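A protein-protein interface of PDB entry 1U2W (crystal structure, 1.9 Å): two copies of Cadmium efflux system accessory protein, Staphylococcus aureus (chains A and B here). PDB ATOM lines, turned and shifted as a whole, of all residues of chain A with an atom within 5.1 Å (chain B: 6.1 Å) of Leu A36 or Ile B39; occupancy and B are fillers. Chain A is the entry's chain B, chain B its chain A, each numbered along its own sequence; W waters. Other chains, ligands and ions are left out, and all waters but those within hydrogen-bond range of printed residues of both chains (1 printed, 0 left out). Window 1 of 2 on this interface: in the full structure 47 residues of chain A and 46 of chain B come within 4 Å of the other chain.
The backbone carbonyl oxygen (O) of Ala B40 lies within hydrogen-bond range of the side-chain hydroxyl (OG) of Ser A33 (3.0 Å).
The backbone NH (N) of Ala B45 lies close to the backbone carbonyl oxygen (O) of Ile B39, at 3.3 Å.
Among the printed residues, merely in contact across the chains: Ala A40 with Lys B37 (3.6 Å), Lys A37 with Ala B40 (3.6 Å), Ile A39 with Leu B36 (3.7 Å), Ala A40 with Leu B36 (3.8 Å), Leu A36 with Ala B40 (3.8 Å), Val A32 with Met B108 (3.9 Å) and Leu A36 with Ile B39 (3.997 Å).
Of the printed residues of chain B, Leu A36 touches Ile B39 and Ala B40.
Of the printed residues of chain A, Ile B39 touches Leu A36 (3.997 Å).
Of the printed residues of chain B, Ala A40 touches Leu B36 (3.8 Å) and Lys B37 (3.6 Å).
Of the printed residues of chain B, Ile A39 touches Leu B36.
Printed residues of chain B within 4 Å of Val A32: Met B108.
Printed residues of chain B within 4 Å of Lys A37: Ala B40.
Of the printed residues of chain A, Leu B36 touches Ile A39 (3.7 Å) and Ala A40 (3.8 Å).
Ala B111 touches none of the printed residues of chain A.
Ile A35 touches none of the printed residues of chain B.
Hydrophobic or aromatic side chains of chain A that line the printed part of chain B: Val A32, Leu A36, Ile A39 and Ala A40.
Of the 19 printed residues of chain B, 5 touch a printed residue of chain A.
Hydrophobic or aromatic side chains of chain B that line the printed part of chain A: Leu B36, Ile B39, Ala B40 and Met B108.
Along chain B the printed residues that touch a printed residue of chain A span positions 36 to 108.
Among the printed residues, 8 pairs touch across the chains.
Leu A36 touches Ile B39, and with the chains exchanged Ile A39 touches Leu B36.
Leu A36 touches Ala B40, and with the chains exchanged Ala A40 touches Leu B36.
Lys A37 touches Ala B40, and with the chains exchanged Ala A40 touches Lys B37.
Positions printed for both chains: 34, 35, 36, 37, 38, 39, 40 and 107.
Water W1 lies within hydrogen-bond range of O of Lys A37 (2.7 Å) and NZ of Lys B37 (2.8 Å).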
ATOM      1  N   GLY A  31      29.311   5.306  21.909  1.00  0.00           N
ATOM      2  CA  GLY A  31      27.942   4.818  21.650  1.00  0.00           C
ATOM      3  C   GLY A  31      26.886   5.611  22.345  1.00  0.00           C
ATOM      4  O   GLY A  31      25.783   5.779  21.824  1.00  0.00           O
ATOM      5  N   VAL A  32      27.215   6.108  23.531  1.00  0.00           N
ATOM      6  CA  VAL A  32      26.324   6.943  24.303  1.00  0.00           C
ATOM      7  C   VAL A  32      26.110   8.250  23.527  1.00  0.00           C
ATOM      8  O   VAL A  32      24.992   8.695  23.337  1.00  0.00           O
ATOM      9  CB  VAL A  32      26.871   7.204  25.712  1.00  0.00           C
ATOM     10  CG1 VAL A  32      26.168   8.407  26.339  1.00  0.00           C
ATOM     11  CG2 VAL A  32      26.763   5.956  26.553  1.00  0.00           C
ATOM     12  N   SER A  33      27.200   8.843  23.041  1.00  0.00           N
ATOM     13  CA  SER A  33      27.127   9.999  22.170  1.00  0.00           C
ATOM     14  C   SER A  33      26.193   9.807  20.925  1.00  0.00           C
ATOM     15  O   SER A  33      25.338  10.667  20.621  1.00  0.00           O
ATOM     16  CB  SER A  33      28.575  10.432  21.786  1.00  0.00           C
ATOM     17  OG  SER A  33      28.577  11.021  20.503  1.00  0.00           O
ATOM     18  N   GLN A  34      26.370   8.692  20.208  1.00  0.00           N
ATOM     19  CA  GLN A  34      25.566   8.391  19.049  1.00  0.00           C
ATOM     20  C   GLN A  34      24.102   8.340  19.426  1.00  0.00           C
ATOM     21  O   GLN A  34      23.311   8.940  18.741  1.00  0.00           O
ATOM     22  CB  GLN A  34      25.971   7.057  18.431  1.00  0.00           C
ATOM     23  CG  GLN A  34      27.232   7.163  17.628  1.00  0.00           C
ATOM     24  CD  GLN A  34      27.792   5.810  17.214  1.00  0.00           C
ATOM     25  OE1 GLN A  34      27.077   4.801  17.173  1.00  0.00           O
ATOM     26  NE2 GLN A  34      29.083   5.778  16.908  1.00  0.00           N
ATOM     27  N   ILE A  35      23.739   7.606  20.481  1.00  0.00           N
ATOM     28  CA  ILE A  35      22.321   7.513  20.785  1.00  0.00           C
ATOM     29  C   ILE A  35      21.721   8.845  21.297  1.00  0.00           C
ATOM     30  O   ILE A  35      20.592   9.184  20.956  1.00  0.00           O
ATOM     31  CB  ILE A  35      21.986   6.390  21.728  1.00  0.00           C
ATOM     32  CG1 ILE A  35      20.476   6.170  21.656  1.00  0.00           C
ATOM     33  CG2 ILE A  35      22.407   6.673  23.169  1.00  0.00           C
ATOM     34  CD1 ILE A  35      20.026   5.095  22.571  1.00  0.00           C
ATOM     35  N   LEU A  36      22.502   9.600  22.090  1.00  0.00           N
ATOM     36  CA  LEU A  36      21.989  10.889  22.587  1.00  0.00           C
ATOM     37  C   LEU A  36      21.846  11.876  21.480  1.00  0.00           C
ATOM     38  O   LEU A  36      20.911  12.692  21.489  1.00  0.00           O
ATOM     39  CB  LEU A  36      22.796  11.427  23.763  1.00  0.00           C
ATOM     40  CG  LEU A  36      22.723  10.521  25.023  1.00  0.00           C
ATOM     41  CD1 LEU A  36      23.544  11.194  26.123  1.00  0.00           C
ATOM     42  CD2 LEU A  36      21.305  10.213  25.501  1.00  0.00           C
ATOM     43  N   LYS A  37      22.769  11.840  20.534  1.00  0.00           N
ATOM     44  CA  LYS A  37      22.688  12.698  19.345  1.00  0.00           C
ATOM     45  C   LYS A  37      21.430  12.385  18.514  1.00  0.00           C
ATOM     46  O   LYS A  37      20.792  13.291  17.958  1.00  0.00           O
ATOM     47  CB  LYS A  37      23.987  12.537  18.523  1.00  0.00           C
ATOM     48  CG  LYS A  37      23.922  12.836  17.065  1.00  0.00           C
ATOM     49  CD  LYS A  37      25.328  12.797  16.394  1.00  0.00           C
ATOM     50  CE  LYS A  37      25.316  13.335  14.909  1.00  0.00           C
ATOM     51  NZ  LYS A  37      23.934  13.521  14.307  1.00  0.00           N
ATOM     52  N   ALA A  38      21.129  11.092  18.379  1.00  0.00           N
ATOM     53  CA  ALA A  38      19.946  10.634  17.650  1.00  0.00           C
ATOM     54  C   ALA A  38      18.675  11.226  18.282  1.00  0.00           C
ATOM     55  O   ALA A  38      17.839  11.775  17.595  1.00  0.00           O
ATOM     56  CB  ALA A  38      19.889   9.074  17.627  1.00  0.00           C
ATOM     57  N   ILE A  39      18.580  11.206  19.604  1.00  0.00           N
ATOM     58  CA  ILE A  39      17.369  11.697  20.268  1.00  0.00           C
ATOM     59  C   ILE A  39      17.317  13.201  20.307  1.00  0.00           C
ATOM     60  O   ILE A  39      16.240  13.743  20.253  1.00  0.00           O
ATOM     61  CB  ILE A  39      17.260  11.170  21.690  1.00  0.00           C
ATOM     62  CG1 ILE A  39      17.217   9.650  21.624  1.00  0.00           C
ATOM     63  CG2 ILE A  39      15.982  11.727  22.424  1.00  0.00           C
ATOM     64  CD1 ILE A  39      17.688   8.979  22.926  1.00  0.00           C
ATOM     65  N   ALA A  40      18.488  13.847  20.418  1.00  0.00           N
ATOM     66  CA  ALA A  40      18.609  15.316  20.563  1.00  0.00           C
ATOM     67  C   ALA A  40      18.075  16.136  19.396  1.00  0.00           C
ATOM     68  O   ALA A  40      17.644  17.293  19.564  1.00  0.00           O
ATOM     69  CB  ALA A  40      20.068  15.679  20.771  1.00  0.00           C
ATOM     70  N   ILE A 107      15.036   8.276  29.817  1.00  0.00           N
ATOM     71  CA  ILE A 107      15.914   9.354  29.317  1.00  0.00           C
ATOM     72  C   ILE A 107      15.108  10.621  28.980  1.00  0.00           C
ATOM     73  O   ILE A 107      15.474  11.731  29.390  1.00  0.00           O
ATOM     74  CB  ILE A 107      16.725   8.899  28.064  1.00  0.00           C
ATOM     75  CG1 ILE A 107      17.788   7.848  28.479  1.00  0.00           C
ATOM     76  CG2 ILE A 107      17.393  10.123  27.349  1.00  0.00           C
ATOM     77  CD1 ILE A 107      18.453   7.166  27.354  1.00  0.00           C
ATOM     78  N   GLN B  34      18.311  20.689  23.774  1.00  0.00           N
ATOM     79  CA  GLN B  34      19.515  21.451  24.148  1.00  0.00           C
ATOM     80  C   GLN B  34      20.350  20.691  25.140  1.00  0.00           C
ATOM     81  O   GLN B  34      21.561  20.631  25.016  1.00  0.00           O
ATOM     82  CB  GLN B  34      19.158  22.807  24.752  1.00  0.00           C
ATOM     83  CG  GLN B  34      18.218  23.630  23.931  1.00  0.00           C
ATOM     84  CD  GLN B  34      17.856  24.958  24.611  1.00  0.00           C
ATOM     85  OE1 GLN B  34      17.240  24.993  25.681  1.00  0.00           O
ATOM     86  NE2 GLN B  34      18.229  26.051  23.978  1.00  0.00           N
ATOM     87  N   ILE B  35      19.691  20.072  26.097  1.00  0.00           N
ATOM     88  CA  ILE B  35      20.380  19.422  27.171  1.00  0.00           C
ATOM     89  C   ILE B  35      21.041  18.124  26.656  1.00  0.00           C
ATOM     90  O   ILE B  35      22.196  17.852  26.977  1.00  0.00           O
ATOM     91  CB  ILE B  35      19.430  19.268  28.400  1.00  0.00           C
ATOM     92  CG1 ILE B  35      20.220  19.163  29.709  1.00  0.00           C
ATOM     93  CG2 ILE B  35      18.455  18.086  28.212  1.00  0.00           C
ATOM     94  CD1 ILE B  35      20.527  17.741  30.079  1.00  0.00           C
ATOM     95  N   LEU B  36      20.309  17.328  25.856  1.00  0.00           N
ATOM     96  CA  LEU B  36      20.874  16.155  25.214  1.00  0.00           C
ATOM     97  C   LEU B  36      22.002  16.453  24.243  1.00  0.00           C
ATOM     98  O   LEU B  36      22.991  15.708  24.200  1.00  0.00           O
ATOM     99  CB  LEU B  36      19.780  15.312  24.535  1.00  0.00           C
ATOM    100  CG  LEU B  36      18.774  14.792  25.576  1.00  0.00           C
ATOM    101  CD1 LEU B  36      17.730  13.815  24.929  1.00  0.00           C
ATOM    102  CD2 LEU B  36      19.453  14.058  26.738  1.00  0.00           C
ATOM    103  N   LYS B  37      21.863  17.541  23.491  1.00  0.00           N
ATOM    104  CA  LYS B  37      22.926  17.990  22.565  1.00  0.00           C
ATOM    105  C   LYS B  37      24.198  18.389  23.318  1.00  0.00           C
ATOM    106  O   LYS B  37      25.321  18.091  22.881  1.00  0.00           O
ATOM    107  CB  LYS B  37      22.453  19.195  21.732  1.00  0.00           C
ATOM    108  CG  LYS B  37      21.709  18.870  20.466  1.00  0.00           C
ATOM    109  CD  LYS B  37      21.559  20.110  19.554  1.00  0.00           C
ATOM    110  CE  LYS B  37      20.733  19.783  18.263  1.00  0.00           C
ATOM    111  NZ  LYS B  37      21.188  18.547  17.479  1.00  0.00           N
ATOM    112  N   ALA B  38      24.029  19.074  24.435  1.00  0.00           N
ATOM    113  CA  ALA B  38      25.174  19.396  25.270  1.00  0.00           C
ATOM    114  C   ALA B  38      25.877  18.114  25.731  1.00  0.00           C
ATOM    115  O   ALA B  38      27.103  18.000  25.586  1.00  0.00           O
ATOM    116  CB  ALA B  38      24.772  20.276  26.469  1.00  0.00           C
ATOM    117  N   ILE B  39      25.135  17.127  26.248  1.00  0.00           N
ATOM    118  CA  ILE B  39      25.789  15.911  26.732  1.00  0.00           C
ATOM    119  C   ILE B  39      26.277  15.038  25.575  1.00  0.00           C
ATOM    120  O   ILE B  39      27.233  14.309  25.727  1.00  0.00           O
ATOM    121  CB  ILE B  39      24.904  15.064  27.727  1.00  0.00           C
ATOM    122  CG1 ILE B  39      24.451  15.893  28.927  1.00  0.00           C
ATOM    123  CG2 ILE B  39      25.679  13.810  28.262  1.00  0.00           C
ATOM    124  CD1 ILE B  39      23.202  15.334  29.512  1.00  0.00           C
ATOM    125  N   ALA B  40      25.642  15.113  24.417  1.00  0.00           N
ATOM    126  CA  ALA B  40      25.932  14.173  23.326  1.00  0.00           C
ATOM    127  C   ALA B  40      27.306  14.402  22.705  1.00  0.00           C
ATOM    128  O   ALA B  40      27.860  13.495  22.129  1.00  0.00           O
ATOM    129  CB  ALA B  40      24.886  14.229  22.267  1.00  0.00           C
ATOM    130  N   ASP B  41      27.863  15.604  22.803  1.00  0.00           N
ATOM    131  CA  ASP B  41      29.185  15.861  22.226  1.00  0.00           C
ATOM    132  C   ASP B  41      30.197  14.864  22.801  1.00  0.00           C
ATOM    133  O   ASP B  41      30.221  14.593  24.016  1.00  0.00           O
ATOM    134  CB  ASP B  41      29.590  17.341  22.434  1.00  0.00           C
ATOM    135  CG  ASP B  41      31.012  17.626  22.009  1.00  0.00           C
ATOM    136  OD1 ASP B  41      31.223  18.064  20.883  1.00  0.00           O
ATOM    137  OD2 ASP B  41      31.920  17.362  22.786  1.00  0.00           O
ATOM    138  N   GLU B  42      30.999  14.263  21.916  1.00  0.00           N
ATOM    139  CA  GLU B  42      31.969  13.258  22.341  1.00  0.00           C
ATOM    140  C   GLU B  42      32.731  13.647  23.600  1.00  0.00           C
ATOM    141  O   GLU B  42      32.747  12.923  24.622  1.00  0.00           O
ATOM    142  CB  GLU B  42      32.978  12.959  21.221  1.00  0.00           C
ATOM    143  CG  GLU B  42      32.364  12.684  19.827  1.00  0.00           C
ATOM    144  CD  GLU B  42      32.169  13.953  19.042  1.00  0.00           C
ATOM    145  OE1 GLU B  42      33.110  14.335  18.281  1.00  0.00           O
ATOM    146  OE2 GLU B  42      31.100  14.586  19.205  1.00  0.00           O
ATOM    147  N   ARG B  44      32.070  16.167  25.775  1.00  0.00           N
ATOM    148  CA  ARG B  44      31.225  16.513  26.918  1.00  0.00           C
ATOM    149  C   ARG B  44      30.664  15.288  27.583  1.00  0.00           C
ATOM    150  O   ARG B  44      30.514  15.197  28.829  1.00  0.00           O
ATOM    151  CB  ARG B  44      30.107  17.494  26.496  1.00  0.00           C
ATOM    152  CG  ARG B  44      30.721  18.862  26.209  1.00  0.00           C
ATOM    153  CD  ARG B  44      29.675  19.936  26.048  1.00  0.00           C
ATOM    154  NE  ARG B  44      28.926  19.821  24.809  1.00  0.00           N
ATOM    155  CZ  ARG B  44      29.271  20.452  23.700  1.00  0.00           C
ATOM    156  NH1 ARG B  44      30.359  21.228  23.681  1.00  0.00           N
ATOM    157  NH2 ARG B  44      28.517  20.323  22.621  1.00  0.00           N
ATOM    158  N   ALA B  45      30.370  14.300  26.748  1.00  0.00           N
ATOM    159  CA  ALA B  45      29.982  13.008  27.273  1.00  0.00           C
ATOM    160  C   ALA B  45      31.108  12.363  28.147  1.00  0.00           C
ATOM    161  O   ALA B  45      30.857  11.831  29.251  1.00  0.00           O
ATOM    162  CB  ALA B  45      29.578  12.123  26.130  1.00  0.00           C
ATOM    163  N   LYS B  46      32.362  12.467  27.678  1.00  0.00           N
ATOM    164  CA  LYS B  46      33.501  12.065  28.503  1.00  0.00           C
ATOM    165  C   LYS B  46      33.595  12.806  29.832  1.00  0.00           C
ATOM    166  O   LYS B  46      33.737  12.179  30.891  1.00  0.00           O
ATOM    167  CB  LYS B  46      34.794  12.218  27.699  1.00  0.00           C
ATOM    168  CG  LYS B  46      34.940  11.131  26.613  1.00  0.00           C
ATOM    169  CD  LYS B  46      36.035  11.605  25.631  1.00  0.00           C
ATOM    170  CE  LYS B  46      36.788  10.442  25.015  1.00  0.00           C
ATOM    171  NZ  LYS B  46      37.911  11.048  24.231  1.00  0.00           N
ATOM    172  N   THR B  48      31.099  14.307  31.403  1.00  0.00           N
ATOM    173  CA  THR B  48      29.973  13.870  32.204  1.00  0.00           C
ATOM    174  C   THR B  48      30.249  12.505  32.841  1.00  0.00           C
ATOM    175  O   THR B  48      30.009  12.282  34.048  1.00  0.00           O
ATOM    176  CB  THR B  48      28.691  13.823  31.290  1.00  0.00           C
ATOM    177  OG1 THR B  48      28.583  15.104  30.660  1.00  0.00           O
ATOM    178  CG2 THR B  48      27.433  13.571  32.103  1.00  0.00           C
ATOM    179  N   LEU B  80      28.284  22.824  29.307  1.00  0.00           N
ATOM    180  CA  LEU B  80      27.648  21.912  30.260  1.00  0.00           C
ATOM    181  C   LEU B  80      26.999  22.699  31.391  1.00  0.00           C
ATOM    182  O   LEU B  80      25.882  22.400  31.816  1.00  0.00           O
ATOM    183  CB  LEU B  80      28.643  20.881  30.788  1.00  0.00           C
ATOM    184  CG  LEU B  80      29.100  19.887  29.717  1.00  0.00           C
ATOM    185  CD1 LEU B  80      30.198  18.914  30.207  1.00  0.00           C
ATOM    186  CD2 LEU B  80      27.901  19.069  29.151  1.00  0.00           C
ATOM    187  N   VAL B  85      24.413  20.669  33.670  1.00  0.00           N
ATOM    188  CA  VAL B  85      24.974  19.316  33.616  1.00  0.00           C
ATOM    189  C   VAL B  85      26.093  19.171  34.624  1.00  0.00           C
ATOM    190  O   VAL B  85      26.284  18.078  35.151  1.00  0.00           O
ATOM    191  CB  VAL B  85      25.478  18.931  32.191  1.00  0.00           C
ATOM    192  CG1 VAL B  85      26.238  17.573  32.207  1.00  0.00           C
ATOM    193  CG2 VAL B  85      24.330  18.885  31.176  1.00  0.00           C
ATOM    194  N   ILE B 104      21.379  13.850  35.706  1.00  0.00           N
ATOM    195  CA  ILE B 104      22.443  13.697  34.724  1.00  0.00           C
ATOM    196  C   ILE B 104      23.154  12.354  34.869  1.00  0.00           C
ATOM    197  O   ILE B 104      23.391  11.672  33.879  1.00  0.00           O
ATOM    198  CB  ILE B 104      23.442  14.882  34.787  1.00  0.00           C
ATOM    199  CG1 ILE B 104      22.652  16.206  34.753  1.00  0.00           C
ATOM    200  CG2 ILE B 104      24.455  14.759  33.642  1.00  0.00           C
ATOM    201  CD1 ILE B 104      21.918  16.492  33.481  1.00  0.00           C
ATOM    202  N   ILE B 107      20.733   9.620  33.416  1.00  0.00           N
ATOM    203  CA  ILE B 107      20.670   9.592  31.939  1.00  0.00           C
ATOM    204  C   ILE B 107      21.929   8.867  31.391  1.00  0.00           C
ATOM    205  O   ILE B 107      21.824   8.052  30.507  1.00  0.00           O
ATOM    206  CB  ILE B 107      20.630  11.039  31.384  1.00  0.00           C
ATOM    207  CG1 ILE B 107      19.216  11.679  31.601  1.00  0.00           C
ATOM    208  CG2 ILE B 107      21.042  11.107  29.859  1.00  0.00           C
ATOM    209  CD1 ILE B 107      19.196  13.210  31.384  1.00  0.00           C
ATOM    210  N   MET B 108      23.128   9.227  31.921  1.00  0.00           N
ATOM    211  CA  MET B 108      24.366   8.565  31.461  1.00  0.00           C
ATOM    212  C   MET B 108      24.299   7.058  31.630  1.00  0.00           C
ATOM    213  O   MET B 108      24.581   6.331  30.692  1.00  0.00           O
ATOM    214  CB  MET B 108      25.617   9.187  32.098  1.00  0.00           C
ATOM    215  CG  MET B 108      26.954   8.480  31.754  1.00  0.00           C
ATOM    216  SD  MET B 108      27.392   8.716  30.024  1.00  0.00           S
ATOM    217  CE  MET B 108      28.691   7.531  29.728  1.00  0.00           C
ATOM    218  N   ALA B 111      21.697   5.338  29.239  1.00  0.00           N
ATOM    219  CA  ALA B 111      22.120   5.250  27.839  1.00  0.00           C
ATOM    220  C   ALA B 111      23.197   4.180  27.680  1.00  0.00           C
ATOM    221  O   ALA B 111      23.189   3.406  26.722  1.00  0.00           O
ATOM    222  CB  ALA B 111      22.603   6.518  27.402  1.00  0.00           C
HETATM  223  O   HOH W   1      21.468  15.805  17.401  1.00  0.00           O
